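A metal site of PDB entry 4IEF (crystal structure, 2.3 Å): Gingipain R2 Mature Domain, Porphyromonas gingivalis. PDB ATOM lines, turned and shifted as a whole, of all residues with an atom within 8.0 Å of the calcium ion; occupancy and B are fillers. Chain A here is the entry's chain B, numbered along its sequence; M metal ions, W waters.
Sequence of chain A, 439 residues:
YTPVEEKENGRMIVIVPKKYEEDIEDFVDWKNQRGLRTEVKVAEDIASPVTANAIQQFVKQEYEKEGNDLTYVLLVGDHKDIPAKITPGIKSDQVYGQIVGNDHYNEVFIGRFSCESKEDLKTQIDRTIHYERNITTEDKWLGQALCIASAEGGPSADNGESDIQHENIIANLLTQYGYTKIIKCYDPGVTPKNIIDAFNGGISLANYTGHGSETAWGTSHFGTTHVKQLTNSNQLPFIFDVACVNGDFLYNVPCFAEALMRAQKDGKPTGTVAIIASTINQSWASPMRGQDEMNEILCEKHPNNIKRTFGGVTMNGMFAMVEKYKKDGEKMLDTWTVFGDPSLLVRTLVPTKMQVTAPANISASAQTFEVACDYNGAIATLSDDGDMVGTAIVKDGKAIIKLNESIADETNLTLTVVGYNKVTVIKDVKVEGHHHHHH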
ATOM      1  N   GLY A  77     -14.920  -6.771  14.394  1.00  0.00           N
ATOM      2  CA  GLY A  77     -16.206  -7.207  13.875  1.00  0.00           C
ATOM      3  C   GLY A  77     -17.155  -6.080  13.539  1.00  0.00           C
ATOM      4  O   GLY A  77     -16.969  -4.947  13.999  1.00  0.00           O
ATOM      5  N   ASP A  78     -18.194  -6.401  12.754  1.00  0.00           N
ATOM      6  CA  ASP A  78     -19.230  -5.432  12.408  1.00  0.00           C
ATOM      7  C   ASP A  78     -20.182  -5.281  13.613  1.00  0.00           C
ATOM      8  O   ASP A  78     -19.940  -5.904  14.661  1.00  0.00           O
ATOM      9  CB  ASP A  78     -19.967  -5.829  11.109  1.00  0.00           C
ATOM     10  CG  ASP A  78     -20.419  -4.644  10.275  1.00  0.00           C
ATOM     11  OD1 ASP A  78     -20.277  -4.712   9.031  1.00  0.00           O
ATOM     12  OD2 ASP A  78     -20.933  -3.659  10.864  1.00  0.00           O
ATOM     13  N   HIS A  79     -21.252  -4.463  13.487  1.00  0.00           N
ATOM     14  CA  HIS A  79     -22.169  -4.184  14.591  1.00  0.00           C
ATOM     15  C   HIS A  79     -22.883  -5.451  15.111  1.00  0.00           C
ATOM     16  O   HIS A  79     -23.126  -5.547  16.307  1.00  0.00           O
ATOM     17  CB  HIS A  79     -23.170  -3.062  14.235  1.00  0.00           C
ATOM     18  CG  HIS A  79     -24.308  -3.464  13.353  1.00  0.00           C
ATOM     19  ND1 HIS A  79     -25.622  -3.430  13.805  1.00  0.00           N
ATOM     20  CD2 HIS A  79     -24.312  -3.847  12.052  1.00  0.00           C
ATOM     21  CE1 HIS A  79     -26.369  -3.809  12.779  1.00  0.00           C
ATOM     22  NE2 HIS A  79     -25.619  -4.082  11.708  1.00  0.00           N
ATOM     23  N   LYS A  80     -23.176  -6.440  14.230  1.00  0.00           N
ATOM     24  CA  LYS A  80     -23.801  -7.708  14.620  1.00  0.00           C
ATOM     25  C   LYS A  80     -22.864  -8.551  15.512  1.00  0.00           C
ATOM     26  O   LYS A  80     -23.351  -9.321  16.336  1.00  0.00           O
ATOM     27  CB  LYS A  80     -24.222  -8.528  13.385  1.00  0.00           C
ATOM     28  CG  LYS A  80     -25.537  -8.080  12.755  1.00  0.00           C
ATOM     29  CD  LYS A  80     -25.950  -9.021  11.624  1.00  0.00           C
ATOM     30  CE  LYS A  80     -27.396  -8.852  11.201  1.00  0.00           C
ATOM     31  NZ  LYS A  80     -28.349  -9.367  12.212  1.00  0.00           N
ATOM     32  N   ARG A 112     -12.061   0.405  15.732  1.00  0.00           N
ATOM     33  CA  ARG A 112     -12.756  -0.786  15.278  1.00  0.00           C
ATOM     34  C   ARG A 112     -12.241  -1.297  13.935  1.00  0.00           C
ATOM     35  O   ARG A 112     -12.099  -0.532  12.981  1.00  0.00           O
ATOM     36  CB  ARG A 112     -14.277  -0.527  15.176  1.00  0.00           C
ATOM     37  CG  ARG A 112     -15.098  -1.774  14.785  1.00  0.00           C
ATOM     38  CD  ARG A 112     -16.549  -1.459  14.513  1.00  0.00           C
ATOM     39  NE  ARG A 112     -17.299  -1.217  15.747  1.00  0.00           N
ATOM     40  CZ  ARG A 112     -18.084  -2.110  16.351  1.00  0.00           C
ATOM     41  NH1 ARG A 112     -18.241  -3.320  15.836  1.00  0.00           N
ATOM     42  NH2 ARG A 112     -18.741  -1.787  17.463  1.00  0.00           N
ATOM     43  N   SER A 114     -13.890  -3.292  11.563  1.00  0.00           N
ATOM     44  CA  SER A 114     -15.215  -3.755  11.147  1.00  0.00           C
ATOM     45  C   SER A 114     -15.078  -4.790  10.041  1.00  0.00           C
ATOM     46  O   SER A 114     -14.538  -4.502   8.973  1.00  0.00           O
ATOM     47  CB  SER A 114     -16.085  -2.575  10.715  1.00  0.00           C
ATOM     48  OG  SER A 114     -17.351  -3.020  10.263  1.00  0.00           O
ATOM     49  N   CYS A 115     -15.547  -6.016  10.298  1.00  0.00           N
ATOM     50  CA  CYS A 115     -15.398  -7.100   9.346  1.00  0.00           C
ATOM     51  C   CYS A 115     -16.602  -8.029   9.321  1.00  0.00           C
ATOM     52  O   CYS A 115     -17.167  -8.329  10.377  1.00  0.00           O
ATOM     53  CB  CYS A 115     -14.123  -7.872   9.638  1.00  0.00           C
ATOM     54  SG  CYS A 115     -13.960  -8.400  11.363  1.00  0.00           S
ATOM     55  N   GLU A 116     -16.960  -8.504   8.128  1.00  0.00           N
ATOM     56  CA  GLU A 116     -18.075  -9.448   7.938  1.00  0.00           C
ATOM     57  C   GLU A 116     -17.567 -10.774   7.338  1.00  0.00           C
ATOM     58  O   GLU A 116     -18.363 -11.666   7.007  1.00  0.00           O
ATOM     59  CB  GLU A 116     -19.160  -8.840   7.055  1.00  0.00           C
ATOM     60  CG  GLU A 116     -19.892  -7.687   7.707  1.00  0.00           C
ATOM     61  CD  GLU A 116     -20.969  -7.081   6.841  1.00  0.00           C
ATOM     62  OE1 GLU A 116     -20.672  -6.137   6.068  1.00  0.00           O
ATOM     63  OE2 GLU A 116     -22.114  -7.590   6.891  1.00  0.00           O
ATOM     64  N   GLY A 247     -19.533   7.115   8.525  1.00  0.00           N
ATOM     65  CA  GLY A 247     -19.139   6.075   9.468  1.00  0.00           C
ATOM     66  C   GLY A 247     -20.302   5.320  10.084  1.00  0.00           C
ATOM     67  O   GLY A 247     -20.116   4.661  11.109  1.00  0.00           O
ATOM     68  N   ASP A 248     -21.503   5.373   9.458  1.00  0.00           N
ATOM     69  CA  ASP A 248     -22.669   4.632   9.945  1.00  0.00           C
ATOM     70  C   ASP A 248     -22.485   3.160   9.543  1.00  0.00           C
ATOM     71  O   ASP A 248     -23.040   2.709   8.531  1.00  0.00           O
ATOM     72  CB  ASP A 248     -23.988   5.234   9.423  1.00  0.00           C
ATOM     73  CG  ASP A 248     -25.256   4.556   9.919  1.00  0.00           C
ATOM     74  OD1 ASP A 248     -25.169   3.793  10.912  1.00  0.00           O
ATOM     75  OD2 ASP A 248     -26.331   4.799   9.334  1.00  0.00           O
ATOM     76  N   PHE A 249     -21.701   2.420  10.351  1.00  0.00           N
ATOM     77  CA  PHE A 249     -21.374   1.019  10.090  1.00  0.00           C
ATOM     78  C   PHE A 249     -22.553   0.091  10.462  1.00  0.00           C
ATOM     79  O   PHE A 249     -22.435  -1.131  10.317  1.00  0.00           O
ATOM     80  CB  PHE A 249     -20.067   0.616  10.806  1.00  0.00           C
ATOM     81  CG  PHE A 249     -20.099   0.612  12.313  1.00  0.00           C
ATOM     82  CD1 PHE A 249     -19.771   1.751  13.029  1.00  0.00           C
ATOM     83  CD2 PHE A 249     -20.405  -0.556  13.010  1.00  0.00           C
ATOM     84  CE1 PHE A 249     -19.782   1.741  14.426  1.00  0.00           C
ATOM     85  CE2 PHE A 249     -20.443  -0.560  14.399  1.00  0.00           C
ATOM     86  CZ  PHE A 249     -20.125   0.592  15.098  1.00  0.00           C
ATOM     87  N   LEU A 250     -23.694   0.668  10.884  1.00  0.00           N
ATOM     88  CA  LEU A 250     -24.933  -0.019  11.234  1.00  0.00           C
ATOM     89  C   LEU A 250     -25.864  -0.094  10.016  1.00  0.00           C
ATOM     90  O   LEU A 250     -26.898  -0.733  10.089  1.00  0.00           O
ATOM     91  CB  LEU A 250     -25.648   0.699  12.393  1.00  0.00           C
ATOM     92  CG  LEU A 250     -25.215   0.326  13.823  1.00  0.00           C
ATOM     93  CD1 LEU A 250     -23.933   1.053  14.222  1.00  0.00           C
ATOM     94  CD2 LEU A 250     -26.314   0.679  14.809  1.00  0.00           C
ATOM     95  N   TYR A 251     -25.484   0.577   8.909  1.00  0.00           N
ATOM     96  CA  TYR A 251     -26.235   0.645   7.647  1.00  0.00           C
ATOM     97  C   TYR A 251     -26.360  -0.745   7.020  1.00  0.00           C
ATOM     98  O   TYR A 251     -25.536  -1.614   7.298  1.00  0.00           O
ATOM     99  CB  TYR A 251     -25.537   1.623   6.683  1.00  0.00           C
ATOM    100  CG  TYR A 251     -26.397   2.144   5.543  1.00  0.00           C
ATOM    101  CD1 TYR A 251     -25.927   2.116   4.229  1.00  0.00           C
ATOM    102  CD2 TYR A 251     -27.648   2.706   5.781  1.00  0.00           C
ATOM    103  CE1 TYR A 251     -26.688   2.636   3.187  1.00  0.00           C
ATOM    104  CE2 TYR A 251     -28.430   3.213   4.736  1.00  0.00           C
ATOM    105  CZ  TYR A 251     -27.936   3.174   3.443  1.00  0.00           C
ATOM    106  OH  TYR A 251     -28.705   3.678   2.426  1.00  0.00           O
ATOM    107  N   ASN A 252     -27.426  -0.972   6.202  1.00  0.00           N
ATOM    108  CA  ASN A 252     -27.745  -2.261   5.575  1.00  0.00           C
ATOM    109  C   ASN A 252     -26.690  -2.732   4.574  1.00  0.00           C
ATOM    110  O   ASN A 252     -26.618  -3.925   4.288  1.00  0.00           O
ATOM    111  CB  ASN A 252     -29.135  -2.237   4.933  1.00  0.00           C
ATOM    112  CG  ASN A 252     -29.307  -1.283   3.780  1.00  0.00           C
ATOM    113  OD1 ASN A 252     -28.684  -0.224   3.677  1.00  0.00           O
ATOM    114  ND2 ASN A 252     -30.182  -1.647   2.881  1.00  0.00           N
ATOM    115  N   VAL A 253     -25.876  -1.814   4.025  1.00  0.00           N
ATOM    116  CA  VAL A 253     -24.773  -2.139   3.118  1.00  0.00           C
ATOM    117  C   VAL A 253     -23.482  -1.579   3.748  1.00  0.00           C
ATOM    118  O   VAL A 253     -23.598  -0.685   4.586  1.00  0.00           O
ATOM    119  CB  VAL A 253     -24.970  -1.684   1.633  1.00  0.00           C
ATOM    120  CG1 VAL A 253     -26.141  -2.414   0.973  1.00  0.00           C
ATOM    121  CG2 VAL A 253     -25.131  -0.180   1.509  1.00  0.00           C
ATOM    122  N   PRO A 254     -22.257  -2.066   3.419  1.00  0.00           N
ATOM    123  CA  PRO A 254     -21.051  -1.475   4.026  1.00  0.00           C
ATOM    124  C   PRO A 254     -20.981   0.034   3.818  1.00  0.00           C
ATOM    125  O   PRO A 254     -21.214   0.515   2.706  1.00  0.00           O
ATOM    126  CB  PRO A 254     -19.903  -2.199   3.297  1.00  0.00           C
ATOM    127  CG  PRO A 254     -20.494  -3.514   2.881  1.00  0.00           C
ATOM    128  CD  PRO A 254     -21.899  -3.157   2.482  1.00  0.00           C
ATOM    129  N   CYS A 255     -20.722   0.788   4.921  1.00  0.00           N
ATOM    130  CA  CYS A 255     -20.618   2.233   4.856  1.00  0.00           C
ATOM    131  C   CYS A 255     -19.294   2.651   4.206  1.00  0.00           C
ATOM    132  O   CYS A 255     -18.396   1.829   4.034  1.00  0.00           O
ATOM    133  CB  CYS A 255     -20.803   2.877   6.240  1.00  0.00           C
ATOM    134  SG  CYS A 255     -19.389   2.693   7.362  1.00  0.00           S
ATOM    135  N   GLU A 258     -16.123   1.663   6.069  1.00  0.00           N
ATOM    136  CA  GLU A 258     -15.958   0.203   6.020  1.00  0.00           C
ATOM    137  C   GLU A 258     -15.406  -0.257   4.665  1.00  0.00           C
ATOM    138  O   GLU A 258     -14.487  -1.065   4.651  1.00  0.00           O
ATOM    139  CB  GLU A 258     -17.280  -0.504   6.295  1.00  0.00           C
ATOM    140  CG  GLU A 258     -17.725  -0.518   7.747  1.00  0.00           C
ATOM    141  CD  GLU A 258     -19.092  -1.146   7.940  1.00  0.00           C
ATOM    142  OE1 GLU A 258     -20.017  -0.827   7.151  1.00  0.00           O
ATOM    143  OE2 GLU A 258     -19.259  -1.927   8.904  1.00  0.00           O
ATOM    144  N   ALA A 259     -15.954   0.263   3.547  1.00  0.00           N
ATOM    145  CA  ALA A 259     -15.485  -0.097   2.186  1.00  0.00           C
ATOM    146  C   ALA A 259     -13.991   0.253   1.993  1.00  0.00           C
ATOM    147  O   ALA A 259     -13.259  -0.539   1.403  1.00  0.00           O
ATOM    148  CB  ALA A 259     -16.333   0.597   1.126  1.00  0.00           C
ATOM    149  N   ARG A 262     -11.818  -2.209   4.217  1.00  0.00           N
ATOM    150  CA  ARG A 262     -11.935  -3.595   3.742  1.00  0.00           C
ATOM    151  C   ARG A 262     -11.439  -3.810   2.296  1.00  0.00           C
ATOM    152  O   ARG A 262     -11.444  -4.958   1.806  1.00  0.00           O
ATOM    153  CB  ARG A 262     -13.415  -4.032   3.809  1.00  0.00           C
ATOM    154  CG  ARG A 262     -13.970  -4.162   5.222  1.00  0.00           C
ATOM    155  CD  ARG A 262     -15.447  -4.458   5.149  1.00  0.00           C
ATOM    156  NE  ARG A 262     -16.081  -4.489   6.465  1.00  0.00           N
ATOM    157  CZ  ARG A 262     -17.365  -4.732   6.663  1.00  0.00           C
ATOM    158  NH1 ARG A 262     -18.178  -4.988   5.636  1.00  0.00           N
ATOM    159  NH2 ARG A 262     -17.868  -4.723   7.890  1.00  0.00           N
ATOM    160  N   PHE A 339     -12.193   4.000  12.640  1.00  0.00           N
ATOM    161  CA  PHE A 339     -12.136   2.774  11.859  1.00  0.00           C
ATOM    162  C   PHE A 339     -10.663   2.502  11.661  1.00  0.00           C
ATOM    163  O   PHE A 339      -9.941   3.338  11.135  1.00  0.00           O
ATOM    164  CB  PHE A 339     -12.908   2.912  10.537  1.00  0.00           C
ATOM    165  CG  PHE A 339     -14.398   3.041  10.715  1.00  0.00           C
ATOM    166  CD1 PHE A 339     -14.990   4.284  10.914  1.00  0.00           C
ATOM    167  CD2 PHE A 339     -15.219   1.912  10.680  1.00  0.00           C
ATOM    168  CE1 PHE A 339     -16.366   4.393  11.083  1.00  0.00           C
ATOM    169  CE2 PHE A 339     -16.601   2.032  10.841  1.00  0.00           C
ATOM    170  CZ  PHE A 339     -17.160   3.271  11.036  1.00  0.00           C
HETATM  171 CA    CA M   1     -21.418  -2.581   8.618  1.00  0.00          CA
HETATM  172  O   HOH W   1     -21.834  -3.709   6.406  1.00  0.00           O
HETATM  173  O   HOH W   2     -23.687  -3.439   8.758  1.00  0.00           O
HETATM  174  O   HOH W   3     -22.703  -0.839   7.299  1.00  0.00           O
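Within 4 Å of the calcium ion: Asp 78, Phe 249 and Glu 258.
The nearest printed residue that does not touch the calcium ion is Arg 262 (4.2 Å).
The side-chain carboxylate of Glu 258 sits close to the guanidinium group of Arg 262 (3.3 Å).
The side-chain hydroxyl (OG) of Ser 114 lies close to the side-chain carboxylate (OE2) of Glu 258 (2.6 Å).
The side-chain sulfur (SG) of Cys 255 sits close to the backbone NH (N) of Glu 258 (3.7 Å).
The side-chain carboxylate (OD1) of Asp 78 sits close to the guanidinium group (NH2) of Arg 262, 2.7 Å away.
The backbone carbonyl oxygen (O) of Cys 115 sits at hydrogen-bond distance from the backbone NH (N) of Asp 78.
The backbone carbonyl oxygen (O) of Asp 78 sits at hydrogen-bond distance from the guanidinium group (NH1) of Arg 112 (3.3 Å).
SG of Cys 255 lies close to N of Phe 249, 3.8 Å away.
The calcium ion is bound by OE2 of Glu 258, 2.3 Å away.
Water W2 is bound to the calcium ion, at 2.4 Å.
The side-chain carboxylate (OD1) of Asp 78 binds the calcium ion (2.5 Å).
O of Phe 249 binds the calcium ion, 2.5 Å away.
Water W1 binds the calcium ion (2.5 Å).
Water W3 binds the calcium ion (2.5 Å).
The side-chain carboxylate (OD2) of Asp 78 is bound to the calcium ion.
The calcium ion is bound by OE1 of Glu 258.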
